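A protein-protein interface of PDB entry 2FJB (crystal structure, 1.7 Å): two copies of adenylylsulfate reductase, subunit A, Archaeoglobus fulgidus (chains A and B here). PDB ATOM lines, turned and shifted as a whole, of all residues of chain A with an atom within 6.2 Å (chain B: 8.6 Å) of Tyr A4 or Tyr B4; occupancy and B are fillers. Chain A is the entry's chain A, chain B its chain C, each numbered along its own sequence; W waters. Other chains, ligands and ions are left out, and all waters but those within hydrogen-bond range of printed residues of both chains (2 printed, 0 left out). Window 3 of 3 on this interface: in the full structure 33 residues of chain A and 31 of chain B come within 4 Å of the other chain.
OH of Tyr A4 sits at hydrogen-bond distance from OD2 of Asp A506 (2.6 Å).
Hydrophobic or aromatic side chains of chain A that line the printed part of chain B: Val A2, Tyr A4 and Trp A515. Among the printed residues, 4 pairs touch across the chains.
Printed residues of chain B within 4 Å of Val A2: Tyr B4. Tyr A4 touches one residue of chain B. No residue of chain B comes within 4 Å of Pro A5. Printed residues of chain B within 4 Å of Asp A506: Glu B228. Printed residues of chain B within 4 Å of Trp A515: Glu B228. Tyr B4 touches two residues of chain A. Of the printed residues of chain A, Glu B228 touches Asp A506 and Trp A515. Asp B564 touches none of the printed residues of chain A. His B566 touches none of the printed residues of chain A. The nearest residue of chain B that does not touch Tyr A4 is Val B2 (5.8 Å).
Val A2 touches Tyr B4, but with the chains exchanged Tyr A4 does not touch Val B2 (5.8 Å). Tyr B4 touches its own counterpart, Tyr A4. Positions printed for both chains: 2, 3, 4, 5, 6, 7, 506, 515 and 563. Of the 4 pairs that touch across the chains among the printed residues, 1 has its exchanged pair printed and touching as well.
Val A2 touches Tyr B4 (CG1 to OH, 3.8 Å). Tyr A4 touches Tyr B4. Asp A506 touches Glu B228. Trp A515 touches Glu B228 (CH2 to CG, 3.97 Å).
Water W1 lies within hydrogen-bond range of the side-chain carboxylate (OE2) of Glu B228 (2.6 Å) and the backbone carbonyl oxygen (O) of Asp A506 (3.3 Å). Water W2 lies within hydrogen-bond range of OH of Tyr A4 (2.7 Å) and O of Val B2 (3.3 Å).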
ATOM      1  N   VAL A   2     -24.866   2.765  26.148  1.00  0.00           N
ATOM      2  CA  VAL A   2     -24.258   3.992  25.569  1.00  0.00           C
ATOM      3  C   VAL A   2     -22.819   4.137  26.057  1.00  0.00           C
ATOM      4  O   VAL A   2     -22.521   3.893  27.228  1.00  0.00           O
ATOM      5  CB  VAL A   2     -25.052   5.250  25.979  1.00  0.00           C
ATOM      6  CG1 VAL A   2     -24.474   6.471  25.291  1.00  0.00           C
ATOM      7  CG2 VAL A   2     -26.529   5.076  25.627  1.00  0.00           C
ATOM      8  N   TYR A   3     -21.927   4.526  25.153  1.00  0.00           N
ATOM      9  CA  TYR A   3     -20.523   4.697  25.502  1.00  0.00           C
ATOM     10  C   TYR A   3     -19.998   6.041  25.022  1.00  0.00           C
ATOM     11  O   TYR A   3     -20.185   6.417  23.866  1.00  0.00           O
ATOM     12  CB  TYR A   3     -19.683   3.572  24.893  1.00  0.00           C
ATOM     13  CG  TYR A   3     -18.207   3.665  25.216  1.00  0.00           C
ATOM     14  CD1 TYR A   3     -17.770   3.782  26.534  1.00  0.00           C
ATOM     15  CD2 TYR A   3     -17.248   3.622  24.203  1.00  0.00           C
ATOM     16  CE1 TYR A   3     -16.414   3.854  26.841  1.00  0.00           C
ATOM     17  CE2 TYR A   3     -15.883   3.693  24.499  1.00  0.00           C
ATOM     18  CZ  TYR A   3     -15.477   3.809  25.821  1.00  0.00           C
ATOM     19  OH  TYR A   3     -14.138   3.876  26.128  1.00  0.00           O
ATOM     20  N   TYR A   4     -19.352   6.765  25.928  1.00  0.00           N
ATOM     21  CA  TYR A   4     -18.777   8.067  25.614  1.00  0.00           C
ATOM     22  C   TYR A   4     -17.319   8.087  26.047  1.00  0.00           C
ATOM     23  O   TYR A   4     -17.000   8.427  27.188  1.00  0.00           O
ATOM     24  CB  TYR A   4     -19.552   9.180  26.323  1.00  0.00           C
ATOM     25  CG  TYR A   4     -20.774   9.639  25.560  1.00  0.00           C
ATOM     26  CD1 TYR A   4     -21.759   8.733  25.172  1.00  0.00           C
ATOM     27  CD2 TYR A   4     -20.939  10.980  25.211  1.00  0.00           C
ATOM     28  CE1 TYR A   4     -22.879   9.147  24.452  1.00  0.00           C
ATOM     29  CE2 TYR A   4     -22.058  11.405  24.490  1.00  0.00           C
ATOM     30  CZ  TYR A   4     -23.024  10.480  24.116  1.00  0.00           C
ATOM     31  OH  TYR A   4     -24.138  10.884  23.411  1.00  0.00           O
ATOM     32  N   PRO A   5     -16.409   7.704  25.137  1.00  0.00           N
ATOM     33  CA  PRO A   5     -14.979   7.688  25.456  1.00  0.00           C
ATOM     34  C   PRO A   5     -14.460   9.069  25.835  1.00  0.00           C
ATOM     35  O   PRO A   5     -14.862  10.079  25.254  1.00  0.00           O
ATOM     36  CB  PRO A   5     -14.345   7.147  24.176  1.00  0.00           C
ATOM     37  CG  PRO A   5     -15.296   7.597  23.108  1.00  0.00           C
ATOM     38  CD  PRO A   5     -16.638   7.316  23.734  1.00  0.00           C
ATOM     39  N   LYS A   6     -13.573   9.094  26.823  1.00  0.00           N
ATOM     40  CA  LYS A   6     -12.976  10.328  27.318  1.00  0.00           C
ATOM     41  C   LYS A   6     -12.067  10.912  26.240  1.00  0.00           C
ATOM     42  O   LYS A   6     -12.012  12.126  26.045  1.00  0.00           O
ATOM     43  CB  LYS A   6     -12.159  10.027  28.579  1.00  0.00           C
ATOM     44  CG  LYS A   6     -12.051  11.171  29.572  1.00  0.00           C
ATOM     45  CD  LYS A   6     -13.216  11.159  30.552  1.00  0.00           C
ATOM     46  CE  LYS A   6     -12.968  12.101  31.726  1.00  0.00           C
ATOM     47  NZ  LYS A   6     -14.022  11.977  32.775  1.00  0.00           N
ATOM     48  N   LYS A   7     -11.354  10.035  25.544  1.00  0.00           N
ATOM     49  CA  LYS A   7     -10.444  10.449  24.483  1.00  0.00           C
ATOM     50  C   LYS A   7     -10.316   9.355  23.431  1.00  0.00           C
ATOM     51  O   LYS A   7     -10.639   8.193  23.686  1.00  0.00           O
ATOM     52  CB  LYS A   7      -9.058  10.761  25.053  1.00  0.00           C
ATOM     53  CG  LYS A   7      -8.494   9.649  25.911  1.00  0.00           C
ATOM     54  CD  LYS A   7      -9.025   9.752  27.329  1.00  0.00           C
ATOM     55  CE  LYS A   7      -9.132   8.392  27.988  1.00  0.00           C
ATOM     56  NZ  LYS A   7     -10.221   7.582  27.371  1.00  0.00           N
ATOM     57  N   ASP A 506     -21.415  10.662  17.679  1.00  0.00           N
ATOM     58  CA  ASP A 506     -22.362   9.550  17.696  1.00  0.00           C
ATOM     59  C   ASP A 506     -23.634   9.706  16.868  1.00  0.00           C
ATOM     60  O   ASP A 506     -24.551   8.897  16.981  1.00  0.00           O
ATOM     61  CB  ASP A 506     -22.728   9.159  19.131  1.00  0.00           C
ATOM     62  CG  ASP A 506     -23.135  10.338  19.975  1.00  0.00           C
ATOM     63  OD1 ASP A 506     -23.689  11.308  19.423  1.00  0.00           O
ATOM     64  OD2 ASP A 506     -22.913  10.279  21.203  1.00  0.00           O
ATOM     65  N   TRP A 515     -22.688   0.492  20.583  1.00  0.00           N
ATOM     66  CA  TRP A 515     -23.876   0.551  21.427  1.00  0.00           C
ATOM     67  C   TRP A 515     -25.139   0.789  20.608  1.00  0.00           C
ATOM     68  O   TRP A 515     -26.217   0.326  20.979  1.00  0.00           O
ATOM     69  CB  TRP A 515     -23.746   1.620  22.528  1.00  0.00           C
ATOM     70  CG  TRP A 515     -23.820   3.064  22.089  1.00  0.00           C
ATOM     71  CD1 TRP A 515     -22.767   3.909  21.876  1.00  0.00           C
ATOM     72  CD2 TRP A 515     -25.007   3.848  21.897  1.00  0.00           C
ATOM     73  NE1 TRP A 515     -23.224   5.172  21.573  1.00  0.00           N
ATOM     74  CE2 TRP A 515     -24.595   5.162  21.578  1.00  0.00           C
ATOM     75  CE3 TRP A 515     -26.381   3.568  21.966  1.00  0.00           C
ATOM     76  CZ2 TRP A 515     -25.506   6.198  21.328  1.00  0.00           C
ATOM     77  CZ3 TRP A 515     -27.291   4.600  21.716  1.00  0.00           C
ATOM     78  CH2 TRP A 515     -26.845   5.899  21.402  1.00  0.00           C
ATOM     79  N   ARG A 563     -14.064   4.226  18.473  1.00  0.00           N
ATOM     80  CA  ARG A 563     -13.239   5.364  18.872  1.00  0.00           C
ATOM     81  C   ARG A 563     -12.015   5.035  19.727  1.00  0.00           C
ATOM     82  O   ARG A 563     -11.116   5.864  19.869  1.00  0.00           O
ATOM     83  CB  ARG A 563     -14.121   6.396  19.576  1.00  0.00           C
ATOM     84  CG  ARG A 563     -15.145   7.018  18.640  1.00  0.00           C
ATOM     85  CD  ARG A 563     -16.280   7.688  19.395  1.00  0.00           C
ATOM     86  NE  ARG A 563     -17.116   6.706  20.082  1.00  0.00           N
ATOM     87  CZ  ARG A 563     -18.205   7.010  20.781  1.00  0.00           C
ATOM     88  NH1 ARG A 563     -18.597   8.275  20.894  1.00  0.00           N
ATOM     89  NH2 ARG A 563     -18.910   6.046  21.360  1.00  0.00           N
ATOM     90  N   VAL B   2     -30.339   9.648  27.992  1.00  0.00           N
ATOM     91  CA  VAL B   2     -29.024   9.963  28.538  1.00  0.00           C
ATOM     92  C   VAL B   2     -28.543  11.329  28.056  1.00  0.00           C
ATOM     93  O   VAL B   2     -28.695  11.680  26.882  1.00  0.00           O
ATOM     94  CB  VAL B   2     -27.985   8.895  28.137  1.00  0.00           C
ATOM     95  CG1 VAL B   2     -26.663   9.180  28.818  1.00  0.00           C
ATOM     96  CG2 VAL B   2     -28.482   7.517  28.533  1.00  0.00           C
ATOM     97  N   TYR B   3     -27.967  12.100  28.972  1.00  0.00           N
ATOM     98  CA  TYR B   3     -27.464  13.427  28.639  1.00  0.00           C
ATOM     99  C   TYR B   3     -26.032  13.619  29.129  1.00  0.00           C
ATOM    100  O   TYR B   3     -25.721  13.336  30.286  1.00  0.00           O
ATOM    101  CB  TYR B   3     -28.369  14.498  29.257  1.00  0.00           C
ATOM    102  CG  TYR B   3     -27.947  15.919  28.948  1.00  0.00           C
ATOM    103  CD1 TYR B   3     -27.740  16.333  27.632  1.00  0.00           C
ATOM    104  CD2 TYR B   3     -27.753  16.847  29.970  1.00  0.00           C
ATOM    105  CE1 TYR B   3     -27.347  17.639  27.339  1.00  0.00           C
ATOM    106  CE2 TYR B   3     -27.358  18.159  29.689  1.00  0.00           C
ATOM    107  CZ  TYR B   3     -27.158  18.544  28.374  1.00  0.00           C
ATOM    108  OH  TYR B   3     -26.770  19.832  28.090  1.00  0.00           O
ATOM    109  N   TYR B   4     -25.164  14.081  28.230  1.00  0.00           N
ATOM    110  CA  TYR B   4     -23.767  14.349  28.561  1.00  0.00           C
ATOM    111  C   TYR B   4     -23.455  15.777  28.126  1.00  0.00           C
ATOM    112  O   TYR B   4     -23.087  16.015  26.974  1.00  0.00           O
ATOM    113  CB  TYR B   4     -22.813  13.412  27.818  1.00  0.00           C
ATOM    114  CG  TYR B   4     -22.997  11.939  28.075  1.00  0.00           C
ATOM    115  CD1 TYR B   4     -23.816  11.168  27.253  1.00  0.00           C
ATOM    116  CD2 TYR B   4     -22.313  11.301  29.109  1.00  0.00           C
ATOM    117  CE1 TYR B   4     -23.943   9.797  27.445  1.00  0.00           C
ATOM    118  CE2 TYR B   4     -22.436   9.926  29.314  1.00  0.00           C
ATOM    119  CZ  TYR B   4     -23.252   9.182  28.476  1.00  0.00           C
ATOM    120  OH  TYR B   4     -23.376   7.823  28.660  1.00  0.00           O
ATOM    121  N   PRO B   5     -23.601  16.745  29.038  1.00  0.00           N
ATOM    122  CA  PRO B   5     -23.323  18.145  28.704  1.00  0.00           C
ATOM    123  C   PRO B   5     -21.865  18.361  28.310  1.00  0.00           C
ATOM    124  O   PRO B   5     -20.965  17.726  28.856  1.00  0.00           O
ATOM    125  CB  PRO B   5     -23.694  18.880  29.987  1.00  0.00           C
ATOM    126  CG  PRO B   5     -23.343  17.878  31.047  1.00  0.00           C
ATOM    127  CD  PRO B   5     -23.906  16.600  30.472  1.00  0.00           C
ATOM    128  N   LYS B   6     -21.650  19.259  27.355  1.00  0.00           N
ATOM    129  CA  LYS B   6     -20.316  19.585  26.862  1.00  0.00           C
ATOM    130  C   LYS B   6     -19.542  20.260  27.990  1.00  0.00           C
ATOM    131  O   LYS B   6     -18.355  20.007  28.188  1.00  0.00           O
ATOM    132  CB  LYS B   6     -20.425  20.539  25.669  1.00  0.00           C
ATOM    133  CG  LYS B   6     -19.343  20.381  24.609  1.00  0.00           C
ATOM    134  CD  LYS B   6     -19.717  19.302  23.598  1.00  0.00           C
ATOM    135  CE  LYS B   6     -18.781  19.325  22.392  1.00  0.00           C
ATOM    136  NZ  LYS B   6     -19.237  18.425  21.293  1.00  0.00           N
ATOM    137  N   LYS B   7     -20.225  21.132  28.723  1.00  0.00           N
ATOM    138  CA  LYS B   7     -19.606  21.818  29.846  1.00  0.00           C
ATOM    139  C   LYS B   7     -20.661  22.237  30.859  1.00  0.00           C
ATOM    140  O   LYS B   7     -21.858  22.181  30.584  1.00  0.00           O
ATOM    141  CB  LYS B   7     -18.806  23.037  29.373  1.00  0.00           C
ATOM    142  CG  LYS B   7     -19.612  24.275  29.037  1.00  0.00           C
ATOM    143  CD  LYS B   7     -20.467  24.096  27.806  1.00  0.00           C
ATOM    144  CE  LYS B   7     -20.869  25.453  27.244  1.00  0.00           C
ATOM    145  NZ  LYS B   7     -21.464  26.343  28.285  1.00  0.00           N
ATOM    146  N   TYR B   8     -20.213  22.649  32.037  1.00  0.00           N
ATOM    147  CA  TYR B   8     -21.123  23.060  33.097  1.00  0.00           C
ATOM    148  C   TYR B   8     -21.654  24.474  32.906  1.00  0.00           C
ATOM    149  O   TYR B   8     -21.005  25.323  32.297  1.00  0.00           O
ATOM    150  CB  TYR B   8     -20.419  22.990  34.451  1.00  0.00           C
ATOM    151  CG  TYR B   8     -19.830  21.645  34.801  1.00  0.00           C
ATOM    152  CD1 TYR B   8     -18.771  21.552  35.702  1.00  0.00           C
ATOM    153  CD2 TYR B   8     -20.332  20.466  34.247  1.00  0.00           C
ATOM    154  CE1 TYR B   8     -18.219  20.325  36.043  1.00  0.00           C
ATOM    155  CE2 TYR B   8     -19.787  19.226  34.584  1.00  0.00           C
ATOM    156  CZ  TYR B   8     -18.728  19.167  35.483  1.00  0.00           C
ATOM    157  OH  TYR B   8     -18.171  17.958  35.831  1.00  0.00           O
ATOM    158  N   GLU B 228     -31.847   5.750  21.137  1.00  0.00           N
ATOM    159  CA  GLU B 228     -32.023   7.090  20.584  1.00  0.00           C
ATOM    160  C   GLU B 228     -33.513   7.317  20.386  1.00  0.00           C
ATOM    161  O   GLU B 228     -34.020   8.414  20.618  1.00  0.00           O
ATOM    162  CB  GLU B 228     -31.351   7.238  19.210  1.00  0.00           C
ATOM    163  CG  GLU B 228     -29.840   7.282  19.193  1.00  0.00           C
ATOM    164  CD  GLU B 228     -29.305   7.694  17.827  1.00  0.00           C
ATOM    165  OE1 GLU B 228     -30.012   7.477  16.818  1.00  0.00           O
ATOM    166  OE2 GLU B 228     -28.179   8.225  17.756  1.00  0.00           O
ATOM    167  N   ASP B 505     -19.300  12.007  36.976  1.00  0.00           N
ATOM    168  CA  ASP B 505     -20.420  12.902  37.257  1.00  0.00           C
ATOM    169  C   ASP B 505     -21.774  12.207  37.328  1.00  0.00           C
ATOM    170  O   ASP B 505     -22.620  12.587  38.137  1.00  0.00           O
ATOM    171  CB  ASP B 505     -20.516  14.001  36.196  1.00  0.00           C
ATOM    172  CG  ASP B 505     -19.447  15.060  36.340  1.00  0.00           C
ATOM    173  OD1 ASP B 505     -18.690  15.026  37.332  1.00  0.00           O
ATOM    174  OD2 ASP B 505     -19.375  15.936  35.453  1.00  0.00           O
ATOM    175  N   ASP B 506     -21.988  11.203  36.481  1.00  0.00           N
ATOM    176  CA  ASP B 506     -23.277  10.518  36.465  1.00  0.00           C
ATOM    177  C   ASP B 506     -23.394   9.231  37.272  1.00  0.00           C
ATOM    178  O   ASP B 506     -24.354   8.482  37.109  1.00  0.00           O
ATOM    179  CB  ASP B 506     -23.748  10.269  35.025  1.00  0.00           C
ATOM    180  CG  ASP B 506     -22.711   9.572  34.176  1.00  0.00           C
ATOM    181  OD1 ASP B 506     -21.905   8.790  34.726  1.00  0.00           O
ATOM    182  OD2 ASP B 506     -22.719   9.796  32.946  1.00  0.00           O
ATOM    183  N   LEU B 513     -29.483  12.132  38.251  1.00  0.00           N
ATOM    184  CA  LEU B 513     -29.607  13.141  37.204  1.00  0.00           C
ATOM    185  C   LEU B 513     -30.987  12.941  36.585  1.00  0.00           C
ATOM    186  O   LEU B 513     -31.582  11.875  36.726  1.00  0.00           O
ATOM    187  CB  LEU B 513     -28.511  12.953  36.158  1.00  0.00           C
ATOM    188  CG  LEU B 513     -27.109  13.311  36.666  1.00  0.00           C
ATOM    189  CD1 LEU B 513     -26.051  12.721  35.760  1.00  0.00           C
ATOM    190  CD2 LEU B 513     -26.976  14.824  36.747  1.00  0.00           C
ATOM    191  N   TRP B 515     -32.131  12.274  33.531  1.00  0.00           N
ATOM    192  CA  TRP B 515     -32.331  11.102  32.687  1.00  0.00           C
ATOM    193  C   TRP B 515     -32.383   9.818  33.506  1.00  0.00           C
ATOM    194  O   TRP B 515     -33.065   8.862  33.131  1.00  0.00           O
ATOM    195  CB  TRP B 515     -31.254  10.998  31.592  1.00  0.00           C
ATOM    196  CG  TRP B 515     -29.861  10.615  32.036  1.00  0.00           C
ATOM    197  CD1 TRP B 515     -28.810  11.460  32.266  1.00  0.00           C
ATOM    198  CD2 TRP B 515     -29.350   9.284  32.208  1.00  0.00           C
ATOM    199  NE1 TRP B 515     -27.674  10.738  32.558  1.00  0.00           N
ATOM    200  CE2 TRP B 515     -27.978   9.402  32.532  1.00  0.00           C
ATOM    201  CE3 TRP B 515     -29.917   8.005  32.119  1.00  0.00           C
ATOM    202  CZ2 TRP B 515     -27.164   8.287  32.763  1.00  0.00           C
ATOM    203  CZ3 TRP B 515     -29.104   6.893  32.349  1.00  0.00           C
ATOM    204  CH2 TRP B 515     -27.741   7.045  32.667  1.00  0.00           C
ATOM    205  N   GLN B 516     -31.689   9.807  34.640  1.00  0.00           N
ATOM    206  CA  GLN B 516     -31.667   8.628  35.498  1.00  0.00           C
ATOM    207  C   GLN B 516     -32.992   8.468  36.225  1.00  0.00           C
ATOM    208  O   GLN B 516     -33.503   7.358  36.361  1.00  0.00           O
ATOM    209  CB  GLN B 516     -30.507   8.729  36.486  1.00  0.00           C
ATOM    210  CG  GLN B 516     -29.177   8.906  35.771  1.00  0.00           C
ATOM    211  CD  GLN B 516     -28.011   9.039  36.720  1.00  0.00           C
ATOM    212  OE1 GLN B 516     -28.094   9.737  37.730  1.00  0.00           O
ATOM    213  NE2 GLN B 516     -26.904   8.384  36.390  1.00  0.00           N
ATOM    214  N   ARG B 563     -26.526  19.805  35.725  1.00  0.00           N
ATOM    215  CA  ARG B 563     -25.231  20.374  35.351  1.00  0.00           C
ATOM    216  C   ARG B 563     -25.265  21.637  34.491  1.00  0.00           C
ATOM    217  O   ARG B 563     -24.238  22.293  34.304  1.00  0.00           O
ATOM    218  CB  ARG B 563     -24.400  19.289  34.667  1.00  0.00           C
ATOM    219  CG  ARG B 563     -24.075  18.122  35.590  1.00  0.00           C
ATOM    220  CD  ARG B 563     -23.663  16.878  34.813  1.00  0.00           C
ATOM    221  NE  ARG B 563     -24.787  16.274  34.095  1.00  0.00           N
ATOM    222  CZ  ARG B 563     -24.700  15.165  33.367  1.00  0.00           C
ATOM    223  NH1 ARG B 563     -23.537  14.530  33.252  1.00  0.00           N
ATOM    224  NH2 ARG B 563     -25.778  14.681  32.757  1.00  0.00           N
ATOM    225  N   ASP B 564     -26.434  21.959  33.946  1.00  0.00           N
ATOM    226  CA  ASP B 564     -26.612  23.170  33.153  1.00  0.00           C
ATOM    227  C   ASP B 564     -28.093  23.525  33.120  1.00  0.00           C
ATOM    228  O   ASP B 564     -28.920  22.786  33.654  1.00  0.00           O
ATOM    229  CB  ASP B 564     -26.029  23.035  31.726  1.00  0.00           C
ATOM    230  CG  ASP B 564     -26.632  21.888  30.920  1.00  0.00           C
ATOM    231  OD1 ASP B 564     -27.711  21.375  31.281  1.00  0.00           O
ATOM    232  OD2 ASP B 564     -26.013  21.514  29.896  1.00  0.00           O
ATOM    233  N   HIS B 566     -30.180  23.504  30.660  1.00  0.00           N
ATOM    234  CA  HIS B 566     -30.940  22.537  29.871  1.00  0.00           C
ATOM    235  C   HIS B 566     -31.358  21.378  30.777  1.00  0.00           C
ATOM    236  O   HIS B 566     -32.522  20.970  30.795  1.00  0.00           O
ATOM    237  CB  HIS B 566     -30.086  22.002  28.717  1.00  0.00           C
ATOM    238  CG  HIS B 566     -30.757  20.929  27.915  1.00  0.00           C
ATOM    239  ND1 HIS B 566     -31.788  21.190  27.037  1.00  0.00           N
ATOM    240  CD2 HIS B 566     -30.563  19.589  27.880  1.00  0.00           C
ATOM    241  CE1 HIS B 566     -32.198  20.056  26.495  1.00  0.00           C
ATOM    242  NE2 HIS B 566     -31.471  19.070  26.990  1.00  0.00           N
ATOM    243  N   GLU B 567     -30.401  20.859  31.536  1.00  0.00           N
ATOM    244  CA  GLU B 567     -30.676  19.753  32.437  1.00  0.00           C
ATOM    245  C   GLU B 567     -31.518  20.179  33.637  1.00  0.00           C
ATOM    246  O   GLU B 567     -32.221  19.357  34.223  1.00  0.00           O
ATOM    247  CB  GLU B 567     -29.366  19.116  32.906  1.00  0.00           C
ATOM    248  CG  GLU B 567     -29.558  17.818  33.679  1.00  0.00           C
ATOM    249  CD  GLU B 567     -28.276  17.023  33.772  1.00  0.00           C
ATOM    250  OE1 GLU B 567     -27.252  17.604  34.182  1.00  0.00           O
ATOM    251  OE2 GLU B 567     -28.290  15.819  33.437  1.00  0.00           O
HETATM  252  O   HOH W   1     -26.517   8.968  19.660  1.00  0.00           O
HETATM  253  O   HOH W   2     -26.275  10.459  24.923  1.00  0.00           O
